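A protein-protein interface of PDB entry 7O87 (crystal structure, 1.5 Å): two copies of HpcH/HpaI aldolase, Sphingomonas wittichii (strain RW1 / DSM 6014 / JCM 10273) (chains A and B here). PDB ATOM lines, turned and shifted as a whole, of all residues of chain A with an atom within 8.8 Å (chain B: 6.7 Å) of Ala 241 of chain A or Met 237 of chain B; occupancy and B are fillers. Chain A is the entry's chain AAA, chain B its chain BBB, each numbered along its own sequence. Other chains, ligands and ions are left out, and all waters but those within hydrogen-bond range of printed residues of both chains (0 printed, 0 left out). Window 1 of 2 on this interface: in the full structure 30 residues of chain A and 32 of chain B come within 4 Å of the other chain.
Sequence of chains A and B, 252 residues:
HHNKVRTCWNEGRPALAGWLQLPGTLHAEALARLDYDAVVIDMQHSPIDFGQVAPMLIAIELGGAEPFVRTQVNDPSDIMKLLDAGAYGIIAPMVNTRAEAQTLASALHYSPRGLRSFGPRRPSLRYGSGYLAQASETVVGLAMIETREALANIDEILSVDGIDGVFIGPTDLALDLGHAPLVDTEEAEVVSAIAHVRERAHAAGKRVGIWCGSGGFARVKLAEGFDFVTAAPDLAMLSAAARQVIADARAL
Printed residues of chain B within 4 Å of Ala 241 of chain A: Met 237.
Printed residues of chain A within 4 Å of Ala 232 of chain B: Val 245 (3.9 Å).
No residue of chain A comes within 4 Å of Ala 236 of chain B.
Of the printed residues of chain A, Ala 242 of chain B touches Leu 34 and Met 237.
Printed residues of chain A within 4 Å of Ala 231 of chain B: Val 245 (3.7 Å).
Printed residues of chain B within 4 Å of Leu 238 of chain A: Asp 234 and Met 237.
The nearest printed residue of chain A that does not touch Met 237 of chain B is Met 237 of chain A (5.4 Å).
The nearest printed residue of chain B that does not touch Arg 243 of chain A is Leu 31 of chain B (6.1 Å).
Among the printed residues, pairs that only touch across the chains: Leu 34 of chain A with Ser 239 of chain B (3.95 Å), Leu 34 of chain A with Ala 242 of chain B (3.6 Å), Asp 234 of chain A with Leu 238 of chain B (3.6 Å), Met 237 of chain A with Leu 238 of chain B (3.8 Å), Met 237 of chain A with Ala 241 of chain B (3.9 Å), Met 237 of chain A with Ala 242 of chain B (3.8 Å), Leu 238 of chain A with Asp 234 of chain B (3.5 Å), Leu 238 of chain A with Met 237 of chain B (3.9 Å), Ala 241 of chain A with Met 237 of chain B (3.998 Å), Ala 242 of chain A with Leu 31 of chain B (3.4 Å), Ala 242 of chain A with Leu 34 of chain B (3.6 Å), Ala 242 of chain A with Met 237 of chain B (3.8 Å), Arg 243 of chain A with Leu 34 of chain B (3.7 Å), Val 245 of chain A with Ala 231 of chain B (3.7 Å), Val 245 of chain A with Ala 232 of chain B (3.9 Å), Val 245 of chain A with Met 237 of chain B (3.8 Å), Ile 246 of chain A with Leu 34 of chain B (3.7 Å) and Ile 246 of chain A with Tyr 36 of chain B (3.6 Å).
Leu 34 of chain A touches Ser 239 of chain B, but with the chains exchanged Ser 239 of chain A does not touch Leu 34 of chain B (4.04 Å).
Asp 234 of chain A touches Leu 238 of chain B, and with the chains exchanged Leu 238 of chain A touches Asp 234 of chain B.
Met 237 of chain A touches Leu 238 of chain B, and with the chains exchanged Leu 238 of chain A touches Met 237 of chain B.
Ala 242 of chain A touches Leu 31 of chain B, but with the chains exchanged Leu 31 of chain A does not touch Ala 242 of chain B (4.1 Å).
11 positions are printed for both chains.
Of the 18 pairs that touch across the chains among the printed residues, 10 have their exchanged pair printed and touching as well.
Of the 18 printed residues of chain B, 11 touch a printed residue of chain A.
Of the 17 printed residues of chain A, 9 touch a printed residue of chain B.
Among the printed residues, 18 pairs touch across the chains.
The backbone NH (N) of Asp 234 of chain B sits at hydrogen-bond distance from the backbone carbonyl oxygen (O) of Trp 19 of chain B, 2.9 Å away.
O of Ala 231 of chain B is in hydrogen-bond range of OH of Tyr 36 of chain B, 2.7 Å away.
The side-chain hydroxyl (OG) of Ser 239 of chain B is in hydrogen-bond range of the backbone carbonyl oxygen (O) of Leu 235 of chain B (2.7 Å).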
ATOM      1  N   LEU A  31      13.648  -2.385   1.243  1.00  0.00           N
ATOM      2  CA  LEU A  31      12.212  -2.009   1.095  1.00  0.00           C
ATOM      3  C   LEU A  31      12.066  -0.884   0.062  1.00  0.00           C
ATOM      4  O   LEU A  31      11.137  -0.941  -0.733  1.00  0.00           O
ATOM      5  CB  LEU A  31      11.616  -1.632   2.457  1.00  0.00           C
ATOM      6  CG  LEU A  31      10.918  -2.794   3.155  1.00  0.00           C
ATOM      7  CD1 LEU A  31      11.795  -4.018   3.163  1.00  0.00           C
ATOM      8  CD2 LEU A  31      10.497  -2.424   4.567  1.00  0.00           C
ATOM      9  N   LEU A  34      11.610  -2.047  -3.464  1.00  0.00           N
ATOM     10  CA  LEU A  34      10.256  -2.563  -3.819  1.00  0.00           C
ATOM     11  C   LEU A  34       9.403  -1.454  -4.434  1.00  0.00           C
ATOM     12  O   LEU A  34       9.905  -0.314  -4.607  1.00  0.00           O
ATOM     13  CB  LEU A  34       9.619  -3.195  -2.586  1.00  0.00           C
ATOM     14  CG  LEU A  34      10.469  -4.272  -1.929  1.00  0.00           C
ATOM     15  CD1 LEU A  34       9.734  -4.884  -0.760  1.00  0.00           C
ATOM     16  CD2 LEU A  34      10.907  -5.336  -2.939  1.00  0.00           C
ATOM     17  N   ASP A 234       7.559  -2.253   9.393  1.00  0.00           N
ATOM     18  CA  ASP A 234       8.598  -3.300   9.218  1.00  0.00           C
ATOM     19  C   ASP A 234       8.518  -4.301  10.394  1.00  0.00           C
ATOM     20  O   ASP A 234       8.459  -5.528  10.144  1.00  0.00           O
ATOM     21  CB  ASP A 234       9.982  -2.649   9.073  1.00  0.00           C
ATOM     22  CG  ASP A 234      10.409  -1.661  10.143  1.00  0.00           C
ATOM     23  OD1 ASP A 234       9.652  -1.427  11.098  1.00  0.00           O
ATOM     24  OD2 ASP A 234      11.546  -1.154  10.011  1.00  0.00           O
ATOM     25  N   LEU A 235       8.461  -3.835  11.642  1.00  0.00           N
ATOM     26  CA  LEU A 235       8.514  -4.754  12.816  1.00  0.00           C
ATOM     27  C   LEU A 235       7.259  -5.644  12.835  1.00  0.00           C
ATOM     28  O   LEU A 235       7.399  -6.845  13.076  1.00  0.00           O
ATOM     29  CB  LEU A 235       8.648  -3.952  14.115  1.00  0.00           C
ATOM     30  CG  LEU A 235       8.503  -4.740  15.416  1.00  0.00           C
ATOM     31  CD1 LEU A 235       9.622  -5.765  15.580  1.00  0.00           C
ATOM     32  CD2 LEU A 235       8.469  -3.800  16.614  1.00  0.00           C
ATOM     33  N   ALA A 236       6.103  -5.083  12.502  1.00  0.00           N
ATOM     34  CA  ALA A 236       4.825  -5.849  12.401  1.00  0.00           C
ATOM     35  C   ALA A 236       4.897  -6.914  11.298  1.00  0.00           C
ATOM     36  O   ALA A 236       4.496  -8.045  11.543  1.00  0.00           O
ATOM     37  CB  ALA A 236       3.677  -4.902  12.179  1.00  0.00           C
ATOM     38  N   MET A 237       5.354  -6.567  10.104  1.00  0.00           N
ATOM     39  CA  MET A 237       5.456  -7.528   8.981  1.00  0.00           C
ATOM     40  C   MET A 237       6.474  -8.610   9.363  1.00  0.00           C
ATOM     41  O   MET A 237       6.208  -9.799   9.145  1.00  0.00           O
ATOM     42  CB  MET A 237       5.909  -6.844   7.699  1.00  0.00           C
ATOM     43  CG  MET A 237       4.940  -5.772   7.225  1.00  0.00           C
ATOM     44  SD  MET A 237       5.256  -5.195   5.582  1.00  0.00           S
ATOM     45  CE  MET A 237       6.827  -4.377   5.805  1.00  0.00           C
ATOM     46  N   LEU A 238       7.597  -8.205   9.968  1.00  0.00           N
ATOM     47  CA  LEU A 238       8.648  -9.191  10.316  1.00  0.00           C
ATOM     48  C   LEU A 238       8.113 -10.144  11.396  1.00  0.00           C
ATOM     49  O   LEU A 238       8.346 -11.355  11.276  1.00  0.00           O
ATOM     50  CB  LEU A 238       9.936  -8.483  10.757  1.00  0.00           C
ATOM     51  CG  LEU A 238      11.056  -9.348  11.359  1.00  0.00           C
ATOM     52  CD1 LEU A 238      11.523 -10.446  10.392  1.00  0.00           C
ATOM     53  CD2 LEU A 238      12.227  -8.460  11.765  1.00  0.00           C
ATOM     54  N   SER A 239       7.478  -9.638  12.440  1.00  0.00           N
ATOM     55  CA  SER A 239       6.943 -10.484  13.551  1.00  0.00           C
ATOM     56  C   SER A 239       5.913 -11.464  12.998  1.00  0.00           C
ATOM     57  O   SER A 239       5.963 -12.654  13.416  1.00  0.00           O
ATOM     58  CB  SER A 239       6.306  -9.665  14.628  1.00  0.00           C
ATOM     59  OG  SER A 239       7.303  -8.989  15.350  1.00  0.00           O
ATOM     60  N   ALA A 240       4.984 -10.981  12.170  1.00  0.00           N
ATOM     61  CA  ALA A 240       3.925 -11.829  11.562  1.00  0.00           C
ATOM     62  C   ALA A 240       4.600 -12.925  10.712  1.00  0.00           C
ATOM     63  O   ALA A 240       4.202 -14.102  10.820  1.00  0.00           O
ATOM     64  CB  ALA A 240       2.972 -11.024  10.717  1.00  0.00           C
ATOM     65  N   ALA A 241       5.570 -12.578   9.870  1.00  0.00           N
ATOM     66  CA  ALA A 241       6.276 -13.554   9.010  1.00  0.00           C
ATOM     67  C   ALA A 241       6.982 -14.596   9.891  1.00  0.00           C
ATOM     68  O   ALA A 241       6.844 -15.800   9.597  1.00  0.00           O
ATOM     69  CB  ALA A 241       7.223 -12.843   8.063  1.00  0.00           C
ATOM     70  N   ALA A 242       7.637 -14.204  11.000  1.00  0.00           N
ATOM     71  CA  ALA A 242       8.351 -15.147  11.886  1.00  0.00           C
ATOM     72  C   ALA A 242       7.335 -16.074  12.537  1.00  0.00           C
ATOM     73  O   ALA A 242       7.596 -17.308  12.611  1.00  0.00           O
ATOM     74  CB  ALA A 242       9.131 -14.440  12.953  1.00  0.00           C
ATOM     75  N   ARG A 243       6.227 -15.511  13.033  1.00  0.00           N
ATOM     76  CA  ARG A 243       5.213 -16.323  13.742  1.00  0.00           C
ATOM     77  C   ARG A 243       4.772 -17.416  12.765  1.00  0.00           C
ATOM     78  O   ARG A 243       4.574 -18.561  13.224  1.00  0.00           O
ATOM     79  CB  ARG A 243       3.985 -15.498  14.155  1.00  0.00           C
ATOM     80  CG  ARG A 243       4.144 -14.785  15.484  1.00  0.00           C
ATOM     81  CD  ARG A 243       2.858 -14.104  15.965  1.00  0.00           C
ATOM     82  NE  ARG A 243       3.140 -13.267  17.126  1.00  0.00           N
ATOM     83  CZ  ARG A 243       3.426 -11.963  17.096  1.00  0.00           C
ATOM     84  NH1 ARG A 243       3.436 -11.281  15.953  1.00  0.00           N
ATOM     85  NH2 ARG A 243       3.683 -11.334  18.235  1.00  0.00           N
ATOM     86  N   GLN A 244       4.549 -17.058  11.503  1.00  0.00           N
ATOM     87  CA  GLN A 244       4.015 -18.008  10.492  1.00  0.00           C
ATOM     88  C   GLN A 244       5.082 -19.060  10.183  1.00  0.00           C
ATOM     89  O   GLN A 244       4.725 -20.236   9.986  1.00  0.00           O
ATOM     90  CB  GLN A 244       3.585 -17.320   9.194  1.00  0.00           C
ATOM     91  CG  GLN A 244       2.891 -18.257   8.207  1.00  0.00           C
ATOM     92  CD  GLN A 244       1.761 -19.042   8.841  1.00  0.00           C
ATOM     93  OE1 GLN A 244       1.656 -20.273   8.725  1.00  0.00           O
ATOM     94  NE2 GLN A 244       0.908 -18.338   9.553  1.00  0.00           N
ATOM     95  N   VAL A 245       6.349 -18.656  10.109  1.00  0.00           N
ATOM     96  CA  VAL A 245       7.452 -19.619   9.826  1.00  0.00           C
ATOM     97  C   VAL A 245       7.518 -20.639  10.953  1.00  0.00           C
ATOM     98  O   VAL A 245       7.674 -21.844  10.677  1.00  0.00           O
ATOM     99  CB  VAL A 245       8.786 -18.894   9.640  1.00  0.00           C
ATOM    100  CG1 VAL A 245       9.984 -19.827   9.740  1.00  0.00           C
ATOM    101  CG2 VAL A 245       8.735 -18.154   8.324  1.00  0.00           C
ATOM    102  N   ILE A 246       7.436 -20.151  12.188  1.00  0.00           N
ATOM    103  CA  ILE A 246       7.528 -21.016  13.395  1.00  0.00           C
ATOM    104  C   ILE A 246       6.334 -21.974  13.410  1.00  0.00           C
ATOM    105  O   ILE A 246       6.569 -23.204  13.691  1.00  0.00           O
ATOM    106  CB  ILE A 246       7.614 -20.164  14.674  1.00  0.00           C
ATOM    107  CG1 ILE A 246       8.992 -19.522  14.823  1.00  0.00           C
ATOM    108  CG2 ILE A 246       7.235 -20.961  15.901  1.00  0.00           C
ATOM    109  CD1 ILE A 246       9.018 -18.365  15.769  1.00  0.00           C
ATOM    110  N   ALA A 247       5.128 -21.439  13.184  1.00  0.00           N
ATOM    111  CA  ALA A 247       3.863 -22.218  13.149  1.00  0.00           C
ATOM    112  C   ALA A 247       4.010 -23.338  12.105  1.00  0.00           C
ATOM    113  O   ALA A 247       3.627 -24.489  12.387  1.00  0.00           O
ATOM    114  CB  ALA A 247       2.684 -21.334  12.836  1.00  0.00           C
ATOM    115  N   ASP A 248       4.576 -23.032  10.945  1.00  0.00           N
ATOM    116  CA  ASP A 248       4.729 -24.036   9.861  1.00  0.00           C
ATOM    117  C   ASP A 248       5.831 -25.024  10.245  1.00  0.00           C
ATOM    118  O   ASP A 248       5.661 -26.232   9.994  1.00  0.00           O
ATOM    119  CB  ASP A 248       4.994 -23.359   8.519  1.00  0.00           C
ATOM    120  CG  ASP A 248       3.771 -22.650   7.951  1.00  0.00           C
ATOM    121  OD1 ASP A 248       2.644 -23.056   8.294  1.00  0.00           O
ATOM    122  OD2 ASP A 248       3.958 -21.707   7.143  1.00  0.00           O
ATOM    123  N   GLY B  18      15.827 -18.591  15.420  1.00  0.00           N
ATOM    124  CA  GLY B  18      15.832 -17.445  14.487  1.00  0.00           C
ATOM    125  C   GLY B  18      17.225 -17.109  13.977  1.00  0.00           C
ATOM    126  O   GLY B  18      18.246 -17.669  14.453  1.00  0.00           O
ATOM    127  N   TRP B  19      17.287 -16.217  12.984  1.00  0.00           N
ATOM    128  CA  TRP B  19      18.505 -15.884  12.219  1.00  0.00           C
ATOM    129  C   TRP B  19      18.449 -14.393  11.861  1.00  0.00           C
ATOM    130  O   TRP B  19      17.557 -14.012  11.082  1.00  0.00           O
ATOM    131  CB  TRP B  19      18.657 -16.786  10.992  1.00  0.00           C
ATOM    132  CG  TRP B  19      20.028 -16.747  10.389  1.00  0.00           C
ATOM    133  CD1 TRP B  19      20.541 -15.835   9.501  1.00  0.00           C
ATOM    134  CD2 TRP B  19      21.086 -17.673  10.669  1.00  0.00           C
ATOM    135  NE1 TRP B  19      21.859 -16.122   9.251  1.00  0.00           N
ATOM    136  CE2 TRP B  19      22.209 -17.257   9.930  1.00  0.00           C
ATOM    137  CE3 TRP B  19      21.179 -18.810  11.481  1.00  0.00           C
ATOM    138  CZ2 TRP B  19      23.402 -17.974   9.956  1.00  0.00           C
ATOM    139  CZ3 TRP B  19      22.362 -19.511  11.507  1.00  0.00           C
ATOM    140  CH2 TRP B  19      23.451 -19.102  10.742  1.00  0.00           C
ATOM    141  N   LEU B  31      11.661 -11.187  18.251  1.00  0.00           N
ATOM    142  CA  LEU B  31      11.742 -12.578  17.697  1.00  0.00           C
ATOM    143  C   LEU B  31      12.091 -13.558  18.825  1.00  0.00           C
ATOM    144  O   LEU B  31      11.506 -14.642  18.899  1.00  0.00           O
ATOM    145  CB  LEU B  31      12.755 -12.611  16.543  1.00  0.00           C
ATOM    146  CG  LEU B  31      12.337 -11.783  15.326  1.00  0.00           C
ATOM    147  CD1 LEU B  31      13.387 -11.820  14.229  1.00  0.00           C
ATOM    148  CD2 LEU B  31      10.993 -12.221  14.798  1.00  0.00           C
ATOM    149  N   LEU B  34       9.079 -14.953  20.609  1.00  0.00           N
ATOM    150  CA  LEU B  34       8.283 -15.973  19.872  1.00  0.00           C
ATOM    151  C   LEU B  34       8.748 -17.366  20.301  1.00  0.00           C
ATOM    152  O   LEU B  34       9.645 -17.455  21.175  1.00  0.00           O
ATOM    153  CB  LEU B  34       8.433 -15.733  18.362  1.00  0.00           C
ATOM    154  CG  LEU B  34       8.026 -14.341  17.879  1.00  0.00           C
ATOM    155  CD1 LEU B  34       8.204 -14.241  16.382  1.00  0.00           C
ATOM    156  CD2 LEU B  34       6.590 -14.029  18.237  1.00  0.00           C
ATOM    157  N   TYR B  36      10.836 -19.498  19.513  1.00  0.00           N
ATOM    158  CA  TYR B  36      12.245 -19.823  19.210  1.00  0.00           C
ATOM    159  C   TYR B  36      12.970 -20.163  20.519  1.00  0.00           C
ATOM    160  O   TYR B  36      12.856 -19.399  21.479  1.00  0.00           O
ATOM    161  CB  TYR B  36      12.951 -18.628  18.554  1.00  0.00           C
ATOM    162  CG  TYR B  36      12.667 -18.332  17.101  1.00  0.00           C
ATOM    163  CD1 TYR B  36      12.690 -19.315  16.113  1.00  0.00           C
ATOM    164  CD2 TYR B  36      12.501 -17.017  16.691  1.00  0.00           C
ATOM    165  CE1 TYR B  36      12.529 -19.003  14.771  1.00  0.00           C
ATOM    166  CE2 TYR B  36      12.355 -16.689  15.359  1.00  0.00           C
ATOM    167  CZ  TYR B  36      12.373 -17.676  14.387  1.00  0.00           C
ATOM    168  OH  TYR B  36      12.204 -17.313  13.065  1.00  0.00           O
ATOM    169  N   GLY B 213      15.159 -21.730   4.759  1.00  0.00           N
ATOM    170  CA  GLY B 213      14.586 -20.503   4.166  1.00  0.00           C
ATOM    171  C   GLY B 213      13.074 -20.455   4.260  1.00  0.00           C
ATOM    172  O   GLY B 213      12.465 -19.438   3.842  1.00  0.00           O
ATOM    173  N   ALA B 231      15.256 -21.011  10.940  1.00  0.00           N
ATOM    174  CA  ALA B 231      14.343 -20.567   9.876  1.00  0.00           C
ATOM    175  C   ALA B 231      13.643 -19.322  10.382  1.00  0.00           C
ATOM    176  O   ALA B 231      13.237 -19.317  11.554  1.00  0.00           O
ATOM    177  CB  ALA B 231      13.353 -21.676   9.595  1.00  0.00           C
ATOM    178  N   ALA B 232      13.555 -18.271   9.551  1.00  0.00           N
ATOM    179  CA  ALA B 232      14.327 -18.036   8.333  1.00  0.00           C
ATOM    180  C   ALA B 232      14.989 -16.662   8.493  1.00  0.00           C
ATOM    181  O   ALA B 232      14.679 -15.965   9.442  1.00  0.00           O
ATOM    182  CB  ALA B 232      13.413 -18.067   7.127  1.00  0.00           C
ATOM    183  N   PRO B 233      15.948 -16.220   7.650  1.00  0.00           N
ATOM    184  CA  PRO B 233      16.621 -14.950   7.914  1.00  0.00           C
ATOM    185  C   PRO B 233      15.670 -13.733   7.990  1.00  0.00           C
ATOM    186  O   PRO B 233      14.786 -13.577   7.133  1.00  0.00           O
ATOM    187  CB  PRO B 233      17.621 -14.800   6.768  1.00  0.00           C
ATOM    188  CG  PRO B 233      17.819 -16.180   6.246  1.00  0.00           C
ATOM    189  CD  PRO B 233      16.522 -16.930   6.508  1.00  0.00           C
ATOM    190  N   ASP B 234      15.908 -12.850   8.961  1.00  0.00           N
ATOM    191  CA  ASP B 234      15.037 -11.665   9.220  1.00  0.00           C
ATOM    192  C   ASP B 234      14.836 -10.871   7.911  1.00  0.00           C
ATOM    193  O   ASP B 234      13.690 -10.578   7.613  1.00  0.00           O
ATOM    194  CB  ASP B 234      15.543 -10.808  10.371  1.00  0.00           C
ATOM    195  CG  ASP B 234      16.983 -10.290  10.302  1.00  0.00           C
ATOM    196  OD1 ASP B 234      17.697 -10.626   9.354  1.00  0.00           O
ATOM    197  OD2 ASP B 234      17.417  -9.618  11.280  1.00  0.00           O
ATOM    198  N   LEU B 235      15.904 -10.481   7.210  1.00  0.00           N
ATOM    199  CA  LEU B 235      15.819  -9.629   5.998  1.00  0.00           C
ATOM    200  C   LEU B 235      14.999 -10.346   4.922  1.00  0.00           C
ATOM    201  O   LEU B 235      14.144  -9.718   4.339  1.00  0.00           O
ATOM    202  CB  LEU B 235      17.230  -9.313   5.488  1.00  0.00           C
ATOM    203  CG  LEU B 235      17.292  -8.515   4.195  1.00  0.00           C
ATOM    204  CD1 LEU B 235      16.548  -7.196   4.322  1.00  0.00           C
ATOM    205  CD2 LEU B 235      18.739  -8.264   3.786  1.00  0.00           C
ATOM    206  N   ALA B 236      15.223 -11.636   4.698  1.00  0.00           N
ATOM    207  CA  ALA B 236      14.425 -12.421   3.714  1.00  0.00           C
ATOM    208  C   ALA B 236      12.933 -12.418   4.089  1.00  0.00           C
ATOM    209  O   ALA B 236      12.070 -12.231   3.201  1.00  0.00           O
ATOM    210  CB  ALA B 236      14.922 -13.836   3.686  1.00  0.00           C
ATOM    211  N   MET B 237      12.620 -12.718   5.353  1.00  0.00           N
ATOM    212  CA  MET B 237      11.214 -12.777   5.837  1.00  0.00           C
ATOM    213  C   MET B 237      10.560 -11.388   5.652  1.00  0.00           C
ATOM    214  O   MET B 237       9.461 -11.291   5.083  1.00  0.00           O
ATOM    215  CB  MET B 237      11.130 -13.211   7.300  1.00  0.00           C
ATOM    216  CG  MET B 237      11.484 -14.674   7.505  1.00  0.00           C
ATOM    217  SD  MET B 237      10.986 -15.253   9.107  1.00  0.00           S
ATOM    218  CE  MET B 237      12.045 -14.291  10.185  1.00  0.00           C
ATOM    219  N   LEU B 238      11.257 -10.314   6.022  1.00  0.00           N
ATOM    220  CA  LEU B 238      10.707  -8.940   5.932  1.00  0.00           C
ATOM    221  C   LEU B 238      10.493  -8.537   4.477  1.00  0.00           C
ATOM    222  O   LEU B 238       9.418  -7.997   4.158  1.00  0.00           O
ATOM    223  CB  LEU B 238      11.705  -8.004   6.628  1.00  0.00           C
ATOM    224  CG  LEU B 238      11.419  -6.510   6.510  1.00  0.00           C
ATOM    225  CD1 LEU B 238      10.006  -6.185   6.994  1.00  0.00           C
ATOM    226  CD2 LEU B 238      12.458  -5.730   7.334  1.00  0.00           C
ATOM    227  N   SER B 239      11.485  -8.754   3.603  1.00  0.00           N
ATOM    228  CA  SER B 239      11.412  -8.462   2.148  1.00  0.00           C
ATOM    229  C   SER B 239      10.199  -9.170   1.511  1.00  0.00           C
ATOM    230  O   SER B 239       9.459  -8.536   0.720  1.00  0.00           O
ATOM    231  CB  SER B 239      12.700  -8.848   1.443  1.00  0.00           C
ATOM    232  OG  SER B 239      13.820  -8.223   2.062  1.00  0.00           O
ATOM    233  N   ALA B 240      10.016 -10.455   1.780  1.00  0.00           N
ATOM    234  CA  ALA B 240       8.926 -11.240   1.151  1.00  0.00           C
ATOM    235  C   ALA B 240       7.573 -10.744   1.673  1.00  0.00           C
ATOM    236  O   ALA B 240       6.607 -10.615   0.852  1.00  0.00           O
ATOM    237  CB  ALA B 240       9.107 -12.706   1.392  1.00  0.00           C
ATOM    238  N   ALA B 241       7.503 -10.416   2.964  1.00  0.00           N
ATOM    239  CA  ALA B 241       6.280  -9.888   3.591  1.00  0.00           C
ATOM    240  C   ALA B 241       5.900  -8.548   2.938  1.00  0.00           C
ATOM    241  O   ALA B 241       4.720  -8.336   2.588  1.00  0.00           O
ATOM    242  CB  ALA B 241       6.507  -9.731   5.072  1.00  0.00           C
ATOM    243  N   ALA B 242       6.870  -7.650   2.763  1.00  0.00           N
ATOM    244  CA  ALA B 242       6.639  -6.307   2.193  1.00  0.00           C
ATOM    245  C   ALA B 242       6.156  -6.476   0.744  1.00  0.00           C
ATOM    246  O   ALA B 242       5.264  -5.753   0.320  1.00  0.00           O
ATOM    247  CB  ALA B 242       7.892  -5.460   2.274  1.00  0.00           C
